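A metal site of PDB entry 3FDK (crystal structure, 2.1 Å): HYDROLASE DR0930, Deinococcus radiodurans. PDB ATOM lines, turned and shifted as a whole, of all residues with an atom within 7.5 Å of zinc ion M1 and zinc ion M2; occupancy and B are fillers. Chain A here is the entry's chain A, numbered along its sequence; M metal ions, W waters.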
ATOM      1  N   HIS A  21     -25.179 -18.481  -2.403  1.00  0.00           N
ATOM      2  CA  HIS A  21     -23.776 -18.094  -2.374  1.00  0.00           C
ATOM      3  C   HIS A  21     -23.059 -18.685  -3.582  1.00  0.00           C
ATOM      4  O   HIS A  21     -22.685 -19.848  -3.572  1.00  0.00           O
ATOM      5  CB  HIS A  21     -23.079 -18.592  -1.101  1.00  0.00           C
ATOM      6  CG  HIS A  21     -21.698 -18.039  -0.913  1.00  0.00           C
ATOM      7  ND1 HIS A  21     -21.314 -17.373   0.230  1.00  0.00           N
ATOM      8  CD2 HIS A  21     -20.612 -18.065  -1.727  1.00  0.00           C
ATOM      9  CE1 HIS A  21     -20.048 -16.997   0.117  1.00  0.00           C
ATOM     10  NE2 HIS A  21     -19.600 -17.406  -1.059  1.00  0.00           N
ATOM     11  N   GLU A  22     -22.871 -17.854  -4.590  1.00  0.00           N
ATOM     12  CA  GLU A  22     -22.170 -18.265  -5.802  1.00  0.00           C
ATOM     13  C   GLU A  22     -21.365 -17.062  -6.294  1.00  0.00           C
ATOM     14  O   GLU A  22     -21.520 -15.950  -5.801  1.00  0.00           O
ATOM     15  CB  GLU A  22     -23.169 -18.680  -6.881  1.00  0.00           C
ATOM     16  CG  GLU A  22     -24.181 -19.729  -6.457  1.00  0.00           C
ATOM     17  CD  GLU A  22     -23.586 -21.112  -6.282  1.00  0.00           C
ATOM     18  OE1 GLU A  22     -22.490 -21.333  -6.819  1.00  0.00           O
ATOM     19  OE2 GLU A  22     -24.214 -21.960  -5.605  1.00  0.00           O
ATOM     20  N   HIS A  23     -20.518 -17.300  -7.291  1.00  0.00           N
ATOM     21  CA  HIS A  23     -19.684 -16.257  -7.852  1.00  0.00           C
ATOM     22  C   HIS A  23     -19.713 -16.301  -9.385  1.00  0.00           C
ATOM     23  O   HIS A  23     -19.124 -17.201  -9.986  1.00  0.00           O
ATOM     24  CB  HIS A  23     -18.240 -16.433  -7.377  1.00  0.00           C
ATOM     25  CG  HIS A  23     -18.057 -16.236  -5.903  1.00  0.00           C
ATOM     26  ND1 HIS A  23     -18.132 -14.999  -5.307  1.00  0.00           N
ATOM     27  CD2 HIS A  23     -17.835 -17.117  -4.904  1.00  0.00           C
ATOM     28  CE1 HIS A  23     -17.971 -15.126  -4.009  1.00  0.00           C
ATOM     29  NE2 HIS A  23     -17.788 -16.410  -3.732  1.00  0.00           N
ATOM     30  N   PHE A  26     -14.961 -13.987 -10.358  1.00  0.00           N
ATOM     31  CA  PHE A  26     -14.201 -13.844  -9.120  1.00  0.00           C
ATOM     32  C   PHE A  26     -12.720 -13.756  -9.443  1.00  0.00           C
ATOM     33  O   PHE A  26     -12.234 -14.413 -10.357  1.00  0.00           O
ATOM     34  CB  PHE A  26     -14.429 -15.061  -8.217  1.00  0.00           C
ATOM     35  CG  PHE A  26     -13.783 -14.934  -6.862  1.00  0.00           C
ATOM     36  CD1 PHE A  26     -14.482 -14.401  -5.778  1.00  0.00           C
ATOM     37  CD2 PHE A  26     -12.464 -15.335  -6.667  1.00  0.00           C
ATOM     38  CE1 PHE A  26     -13.880 -14.267  -4.538  1.00  0.00           C
ATOM     39  CE2 PHE A  26     -11.847 -15.203  -5.419  1.00  0.00           C
ATOM     40  CZ  PHE A  26     -12.563 -14.668  -4.353  1.00  0.00           C
ATOM     41  N   ASP A  66     -24.939 -13.434  -5.542  1.00  0.00           N
ATOM     42  CA  ASP A  66     -23.518 -13.381  -5.857  1.00  0.00           C
ATOM     43  C   ASP A  66     -22.809 -12.805  -4.632  1.00  0.00           C
ATOM     44  O   ASP A  66     -23.034 -11.655  -4.249  1.00  0.00           O
ATOM     45  CB  ASP A  66     -23.279 -12.484  -7.063  1.00  0.00           C
ATOM     46  CG  ASP A  66     -21.830 -12.448  -7.463  1.00  0.00           C
ATOM     47  OD1 ASP A  66     -21.029 -11.808  -6.744  1.00  0.00           O
ATOM     48  OD2 ASP A  66     -21.488 -13.074  -8.497  1.00  0.00           O
ATOM     49  N   ALA A  67     -21.957 -13.616  -4.006  1.00  0.00           N
ATOM     50  CA  ALA A  67     -21.258 -13.237  -2.784  1.00  0.00           C
ATOM     51  C   ALA A  67     -19.904 -12.558  -2.932  1.00  0.00           C
ATOM     52  O   ALA A  67     -19.188 -12.351  -1.949  1.00  0.00           O
ATOM     53  CB  ALA A  67     -21.109 -14.464  -1.904  1.00  0.00           C
ATOM     54  N   THR A  68     -19.551 -12.194  -4.157  1.00  0.00           N
ATOM     55  CA  THR A  68     -18.250 -11.593  -4.411  1.00  0.00           C
ATOM     56  C   THR A  68     -17.962 -10.287  -3.654  1.00  0.00           C
ATOM     57  O   THR A  68     -18.657  -9.298  -3.844  1.00  0.00           O
ATOM     58  CB  THR A  68     -18.062 -11.307  -5.907  1.00  0.00           C
ATOM     59  OG1 THR A  68     -18.523 -12.444  -6.656  1.00  0.00           O
ATOM     60  CG2 THR A  68     -16.601 -11.060  -6.203  1.00  0.00           C
ATOM     61  N   PRO A  69     -16.924 -10.281  -2.813  1.00  0.00           N
ATOM     62  CA  PRO A  69     -16.569  -9.075  -2.058  1.00  0.00           C
ATOM     63  C   PRO A  69     -16.058  -7.977  -2.995  1.00  0.00           C
ATOM     64  O   PRO A  69     -15.577  -8.255  -4.101  1.00  0.00           O
ATOM     65  CB  PRO A  69     -15.460  -9.563  -1.117  1.00  0.00           C
ATOM     66  CG  PRO A  69     -15.706 -11.058  -0.996  1.00  0.00           C
ATOM     67  CD  PRO A  69     -16.095 -11.437  -2.404  1.00  0.00           C
ATOM     68  N   TYR A  97     -13.252  -8.919   1.733  1.00  0.00           N
ATOM     69  CA  TYR A  97     -12.928 -10.292   2.058  1.00  0.00           C
ATOM     70  C   TYR A  97     -12.154 -10.365   3.370  1.00  0.00           C
ATOM     71  O   TYR A  97     -11.730  -9.343   3.909  1.00  0.00           O
ATOM     72  CB  TYR A  97     -12.120 -10.909   0.906  1.00  0.00           C
ATOM     73  CG  TYR A  97     -12.195 -12.416   0.781  1.00  0.00           C
ATOM     74  CD1 TYR A  97     -13.402 -13.098   0.959  1.00  0.00           C
ATOM     75  CD2 TYR A  97     -11.072 -13.146   0.399  1.00  0.00           C
ATOM     76  CE1 TYR A  97     -13.483 -14.483   0.746  1.00  0.00           C
ATOM     77  CE2 TYR A  97     -11.143 -14.511   0.186  1.00  0.00           C
ATOM     78  CZ  TYR A  97     -12.341 -15.173   0.353  1.00  0.00           C
ATOM     79  OH  TYR A  97     -12.391 -16.533   0.136  1.00  0.00           O
ATOM     80  N   TYR A  98     -11.975 -11.572   3.902  1.00  0.00           N
ATOM     81  CA  TYR A  98     -11.276 -11.734   5.162  1.00  0.00           C
ATOM     82  C   TYR A  98      -9.813 -11.332   5.051  1.00  0.00           C
ATOM     83  O   TYR A  98      -9.241 -11.287   3.959  1.00  0.00           O
ATOM     84  CB  TYR A  98     -11.447 -13.163   5.698  1.00  0.00           C
ATOM     85  CG  TYR A  98     -10.577 -14.239   5.093  1.00  0.00           C
ATOM     86  CD1 TYR A  98      -9.521 -14.776   5.807  1.00  0.00           C
ATOM     87  CD2 TYR A  98     -10.840 -14.755   3.815  1.00  0.00           C
ATOM     88  CE1 TYR A  98      -8.756 -15.819   5.298  1.00  0.00           C
ATOM     89  CE2 TYR A  98     -10.084 -15.804   3.297  1.00  0.00           C
ATOM     90  CZ  TYR A  98      -9.044 -16.332   4.044  1.00  0.00           C
ATOM     91  OH  TYR A  98      -8.288 -17.360   3.557  1.00  0.00           O
ATOM     92  N   KCX A 143     -21.731  -8.721   2.636  1.00  0.00           N
ATOM     93  CA  KCX A 143     -20.866  -9.886   2.757  1.00  0.00           C
ATOM     94  CB  KCX A 143     -20.194 -10.201   1.410  1.00  0.00           C
ATOM     95  CG  KCX A 143     -19.070 -11.254   1.445  1.00  0.00           C
ATOM     96  CD  KCX A 143     -19.563 -12.657   1.817  1.00  0.00           C
ATOM     97  CE  KCX A 143     -18.445 -13.688   1.742  1.00  0.00           C
ATOM     98  NZ  KCX A 143     -18.123 -14.003   0.365  1.00  0.00           N
ATOM     99  C   KCX A 143     -19.795  -9.644   3.821  1.00  0.00           C
ATOM    100  O   KCX A 143     -19.075  -8.655   3.761  1.00  0.00           O
ATOM    101  CX  KCX A 143     -17.450 -15.114   0.019  1.00  0.00           C
ATOM    102  OQ1 KCX A 143     -17.244 -15.266  -1.247  1.00  0.00           O
ATOM    103  OQ2 KCX A 143     -17.045 -15.987   0.880  1.00  0.00           O
ATOM    104  N   LEU A 144     -19.691 -10.560   4.785  1.00  0.00           N
ATOM    105  CA  LEU A 144     -18.679 -10.488   5.833  1.00  0.00           C
ATOM    106  C   LEU A 144     -17.816 -11.745   5.770  1.00  0.00           C
ATOM    107  O   LEU A 144     -18.291 -12.797   5.349  1.00  0.00           O
ATOM    108  CB  LEU A 144     -19.350 -10.395   7.216  1.00  0.00           C
ATOM    109  CG  LEU A 144     -20.140  -9.127   7.521  1.00  0.00           C
ATOM    110  CD1 LEU A 144     -20.846  -9.286   8.872  1.00  0.00           C
ATOM    111  CD2 LEU A 144     -19.209  -7.922   7.547  1.00  0.00           C
ATOM    112  N   ALA A 145     -16.578 -11.647   6.231  1.00  0.00           N
ATOM    113  CA  ALA A 145     -15.673 -12.788   6.215  1.00  0.00           C
ATOM    114  C   ALA A 145     -14.649 -12.704   7.333  1.00  0.00           C
ATOM    115  O   ALA A 145     -14.127 -11.636   7.626  1.00  0.00           O
ATOM    116  CB  ALA A 145     -14.945 -12.867   4.865  1.00  0.00           C
ATOM    117  N   THR A 175     -22.096 -14.598   5.249  1.00  0.00           N
ATOM    118  CA  THR A 175     -20.693 -14.583   5.582  1.00  0.00           C
ATOM    119  C   THR A 175     -19.867 -15.725   5.022  1.00  0.00           C
ATOM    120  O   THR A 175     -20.373 -16.679   4.456  1.00  0.00           O
ATOM    121  CB  THR A 175     -20.464 -14.648   7.094  1.00  0.00           C
ATOM    122  OG1 THR A 175     -20.618 -16.000   7.529  1.00  0.00           O
ATOM    123  CG2 THR A 175     -21.459 -13.764   7.834  1.00  0.00           C
ATOM    124  N   HIS A 176     -18.569 -15.576   5.263  1.00  0.00           N
ATOM    125  CA  HIS A 176     -17.545 -16.536   4.880  1.00  0.00           C
ATOM    126  C   HIS A 176     -16.843 -16.942   6.164  1.00  0.00           C
ATOM    127  O   HIS A 176     -16.373 -16.092   6.915  1.00  0.00           O
ATOM    128  CB  HIS A 176     -16.521 -15.856   3.951  1.00  0.00           C
ATOM    129  CG  HIS A 176     -15.217 -16.595   3.826  1.00  0.00           C
ATOM    130  ND1 HIS A 176     -14.894 -17.339   2.711  1.00  0.00           N
ATOM    131  CD2 HIS A 176     -14.153 -16.671   4.661  1.00  0.00           C
ATOM    132  CE1 HIS A 176     -13.672 -17.835   2.857  1.00  0.00           C
ATOM    133  NE2 HIS A 176     -13.203 -17.450   4.021  1.00  0.00           N
ATOM    134  N   THR A 177     -16.779 -18.240   6.428  1.00  0.00           N
ATOM    135  CA  THR A 177     -16.032 -18.708   7.582  1.00  0.00           C
ATOM    136  C   THR A 177     -14.871 -19.462   6.933  1.00  0.00           C
ATOM    137  O   THR A 177     -15.051 -20.197   5.961  1.00  0.00           O
ATOM    138  CB  THR A 177     -16.843 -19.677   8.475  1.00  0.00           C
ATOM    139  OG1 THR A 177     -17.347 -20.766   7.693  1.00  0.00           O
ATOM    140  CG2 THR A 177     -17.997 -18.945   9.143  1.00  0.00           C
ATOM    141  N   GLN A 178     -13.673 -19.239   7.462  1.00  0.00           N
ATOM    142  CA  GLN A 178     -12.471 -19.864   6.941  1.00  0.00           C
ATOM    143  C   GLN A 178     -12.171 -21.200   7.614  1.00  0.00           C
ATOM    144  O   GLN A 178     -12.101 -21.287   8.845  1.00  0.00           O
ATOM    145  CB  GLN A 178     -11.282 -18.925   7.125  1.00  0.00           C
ATOM    146  CG  GLN A 178      -9.959 -19.407   6.529  1.00  0.00           C
ATOM    147  CD  GLN A 178     -10.001 -19.592   5.015  1.00  0.00           C
ATOM    148  OE1 GLN A 178     -10.814 -18.970   4.318  1.00  0.00           O
ATOM    149  NE2 GLN A 178      -9.126 -20.434   4.505  1.00  0.00           N
ATOM    150  N   GLY A 203     -22.033 -18.473   6.462  1.00  0.00           N
ATOM    151  CA  GLY A 203     -21.582 -19.339   5.386  1.00  0.00           C
ATOM    152  C   GLY A 203     -20.470 -20.343   5.637  1.00  0.00           C
ATOM    153  O   GLY A 203     -19.830 -20.369   6.686  1.00  0.00           O
ATOM    154  N   HIS A 204     -20.244 -21.189   4.624  1.00  0.00           N
ATOM    155  CA  HIS A 204     -19.219 -22.217   4.644  1.00  0.00           C
ATOM    156  C   HIS A 204     -19.255 -23.089   5.892  1.00  0.00           C
ATOM    157  O   HIS A 204     -18.227 -23.621   6.318  1.00  0.00           O
ATOM    158  CB  HIS A 204     -17.824 -21.593   4.478  1.00  0.00           C
ATOM    159  CG  HIS A 204     -17.727 -20.636   3.335  1.00  0.00           C
ATOM    160  ND1 HIS A 204     -18.553 -20.708   2.229  1.00  0.00           N
ATOM    161  CD2 HIS A 204     -16.914 -19.578   3.111  1.00  0.00           C
ATOM    162  CE1 HIS A 204     -18.251 -19.734   1.390  1.00  0.00           C
ATOM    163  NE2 HIS A 204     -17.258 -19.031   1.900  1.00  0.00           N
ATOM    164  N   ASP A 227     -22.701 -24.118   1.786  1.00  0.00           N
ATOM    165  CA  ASP A 227     -22.533 -23.467   0.494  1.00  0.00           C
ATOM    166  C   ASP A 227     -21.320 -23.771  -0.365  1.00  0.00           C
ATOM    167  O   ASP A 227     -20.983 -22.980  -1.254  1.00  0.00           O
ATOM    168  CB  ASP A 227     -22.652 -21.951   0.658  1.00  0.00           C
ATOM    169  CG  ASP A 227     -21.761 -21.396   1.766  1.00  0.00           C
ATOM    170  OD1 ASP A 227     -20.761 -22.059   2.152  1.00  0.00           O
ATOM    171  OD2 ASP A 227     -22.055 -20.288   2.248  1.00  0.00           O
ATOM    172  N   ARG A 228     -20.665 -24.891  -0.092  1.00  0.00           N
ATOM    173  CA  ARG A 228     -19.504 -25.296  -0.875  1.00  0.00           C
ATOM    174  C   ARG A 228     -19.685 -26.746  -1.277  1.00  0.00           C
ATOM    175  O   ARG A 228     -18.711 -27.495  -1.435  1.00  0.00           O
ATOM    176  CB  ARG A 228     -18.220 -25.120  -0.065  1.00  0.00           C
ATOM    177  CG  ARG A 228     -17.793 -23.669   0.049  1.00  0.00           C
ATOM    178  CD  ARG A 228     -16.478 -23.511   0.793  1.00  0.00           C
ATOM    179  NE  ARG A 228     -15.887 -22.220   0.485  1.00  0.00           N
ATOM    180  CZ  ARG A 228     -14.776 -21.737   1.044  1.00  0.00           C
ATOM    181  NH1 ARG A 228     -14.123 -22.448   1.954  1.00  0.00           N
ATOM    182  NH2 ARG A 228     -14.309 -20.558   0.671  1.00  0.00           N
ATOM    183  N   HIS A 263     -23.021 -23.752  -3.778  1.00  0.00           N
ATOM    184  CA  HIS A 263     -21.726 -24.346  -4.180  1.00  0.00           C
ATOM    185  C   HIS A 263     -20.480 -23.457  -4.056  1.00  0.00           C
ATOM    186  O   HIS A 263     -19.355 -23.969  -4.069  1.00  0.00           O
ATOM    187  CB  HIS A 263     -21.752 -24.804  -5.653  1.00  0.00           C
ATOM    188  CG  HIS A 263     -23.028 -25.432  -6.090  1.00  0.00           C
ATOM    189  ND1 HIS A 263     -24.110 -24.708  -6.544  1.00  0.00           N
ATOM    190  CD2 HIS A 263     -23.373 -26.743  -6.203  1.00  0.00           C
ATOM    191  CE1 HIS A 263     -25.063 -25.539  -6.921  1.00  0.00           C
ATOM    192  NE2 HIS A 263     -24.635 -26.774  -6.729  1.00  0.00           N
ATOM    193  N   ASP A 264     -20.666 -22.146  -3.988  1.00  0.00           N
ATOM    194  CA  ASP A 264     -19.548 -21.212  -3.895  1.00  0.00           C
ATOM    195  C   ASP A 264     -18.747 -21.393  -5.197  1.00  0.00           C
ATOM    196  O   ASP A 264     -17.522 -21.319  -5.200  1.00  0.00           O
ATOM    197  CB  ASP A 264     -18.652 -21.519  -2.687  1.00  0.00           C
ATOM    198  CG  ASP A 264     -17.719 -20.359  -2.319  1.00  0.00           C
ATOM    199  OD1 ASP A 264     -17.920 -19.228  -2.789  1.00  0.00           O
ATOM    200  OD2 ASP A 264     -16.776 -20.598  -1.541  1.00  0.00           O
ATOM    201  N   SER A 265     -19.468 -21.641  -6.281  1.00  0.00           N
ATOM    202  CA  SER A 265     -18.824 -21.831  -7.571  1.00  0.00           C
ATOM    203  C   SER A 265     -18.333 -20.505  -8.146  1.00  0.00           C
ATOM    204  O   SER A 265     -18.724 -19.428  -7.711  1.00  0.00           O
ATOM    205  CB  SER A 265     -19.805 -22.463  -8.546  1.00  0.00           C
ATOM    206  OG  SER A 265     -20.860 -21.572  -8.858  1.00  0.00           O
ATOM    207  N   ILE A 266     -17.461 -20.596  -9.143  1.00  0.00           N
ATOM    208  CA  ILE A 266     -16.929 -19.416  -9.809  1.00  0.00           C
ATOM    209  C   ILE A 266     -17.127 -19.739 -11.283  1.00  0.00           C
ATOM    210  O   ILE A 266     -16.462 -20.642 -11.805  1.00  0.00           O
ATOM    211  CB  ILE A 266     -15.437 -19.212  -9.514  1.00  0.00           C
ATOM    212  CG1 ILE A 266     -15.282 -18.820  -8.041  1.00  0.00           C
ATOM    213  CG2 ILE A 266     -14.865 -18.157 -10.440  1.00  0.00           C
ATOM    214  CD1 ILE A 266     -13.876 -18.956  -7.519  1.00  0.00           C
HETATM  215 ZN    ZN M   1     -16.073 -17.551   1.077  1.00  0.00          ZN
HETATM  216 ZN    ZN M   2     -17.588 -17.315  -1.933  1.00  0.00          ZN
HETATM  217  O   HOH W   1     -16.247 -18.094  -0.993  1.00  0.00           O
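Tyr 97 touches zinc ion M1.
Arg 228 touches zinc ion M1 (NH2 to ZN, 3.5 Å).
Five residues have an atom within 4 Å of zinc ion M1: Tyr 97, KCX 143, His 176, His 204 and Arg 228.
The nearest printed residue that does not touch zinc ion M1 is Asp 264 (4.1 Å).
Zinc ion M2 is bound by water W1, at 1.8 Å.
Zinc ion M2 is bound by a ring nitrogen (NE2) of His 23 (2.0 Å).
The side-chain carboxylate (OD1) of Asp 264 binds zinc ion M2 (2.1 Å).
OQ1 of KCX 143 binds zinc ion M2 (2.2 Å).
NE2 of His 21 binds zinc ion M2.
Zinc ion M2 has five donor atoms within binding distance.
Zinc ion M1 is bound by OQ2 of KCX 143 (1.9 Å), ND1 of His 176 (2.0 Å), NE2 of His 204 (2.1 Å) and water W1 (2.1 Å).
The guanidinium group (NE) of Arg 228 lies within salt-bridge range of the side-chain carboxylate (OD2) of Asp 264 (2.7 Å).
The backbone carbonyl oxygen of Leu 144 lies within hydrogen-bond range of the backbone NH of His 176.
O of Ser 265 sits at hydrogen-bond distance from N of His 23, at 2.8 Å.
NZ of KCX 143 sits at hydrogen-bond distance from the backbone carbonyl oxygen (O) of Ala 67 (3.0 Å).
OG1 of Thr 68 lies within hydrogen-bond range of ND1 of His 23, at 2.9 Å.
The side-chain hydroxyl of Thr 177 lies within hydrogen-bond range of the backbone carbonyl oxygen of His 204, at 3.3 Å.
The backbone NH of Asp 264 lies within hydrogen-bond range of the backbone carbonyl oxygen of Asp 227 (2.9 Å).
ND1 of His 204 lies within hydrogen-bond range of OD1 of Asp 227 (2.6 Å).
The nearest printed residue that does not touch zinc ion M2 is His 204 (4.2 Å).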
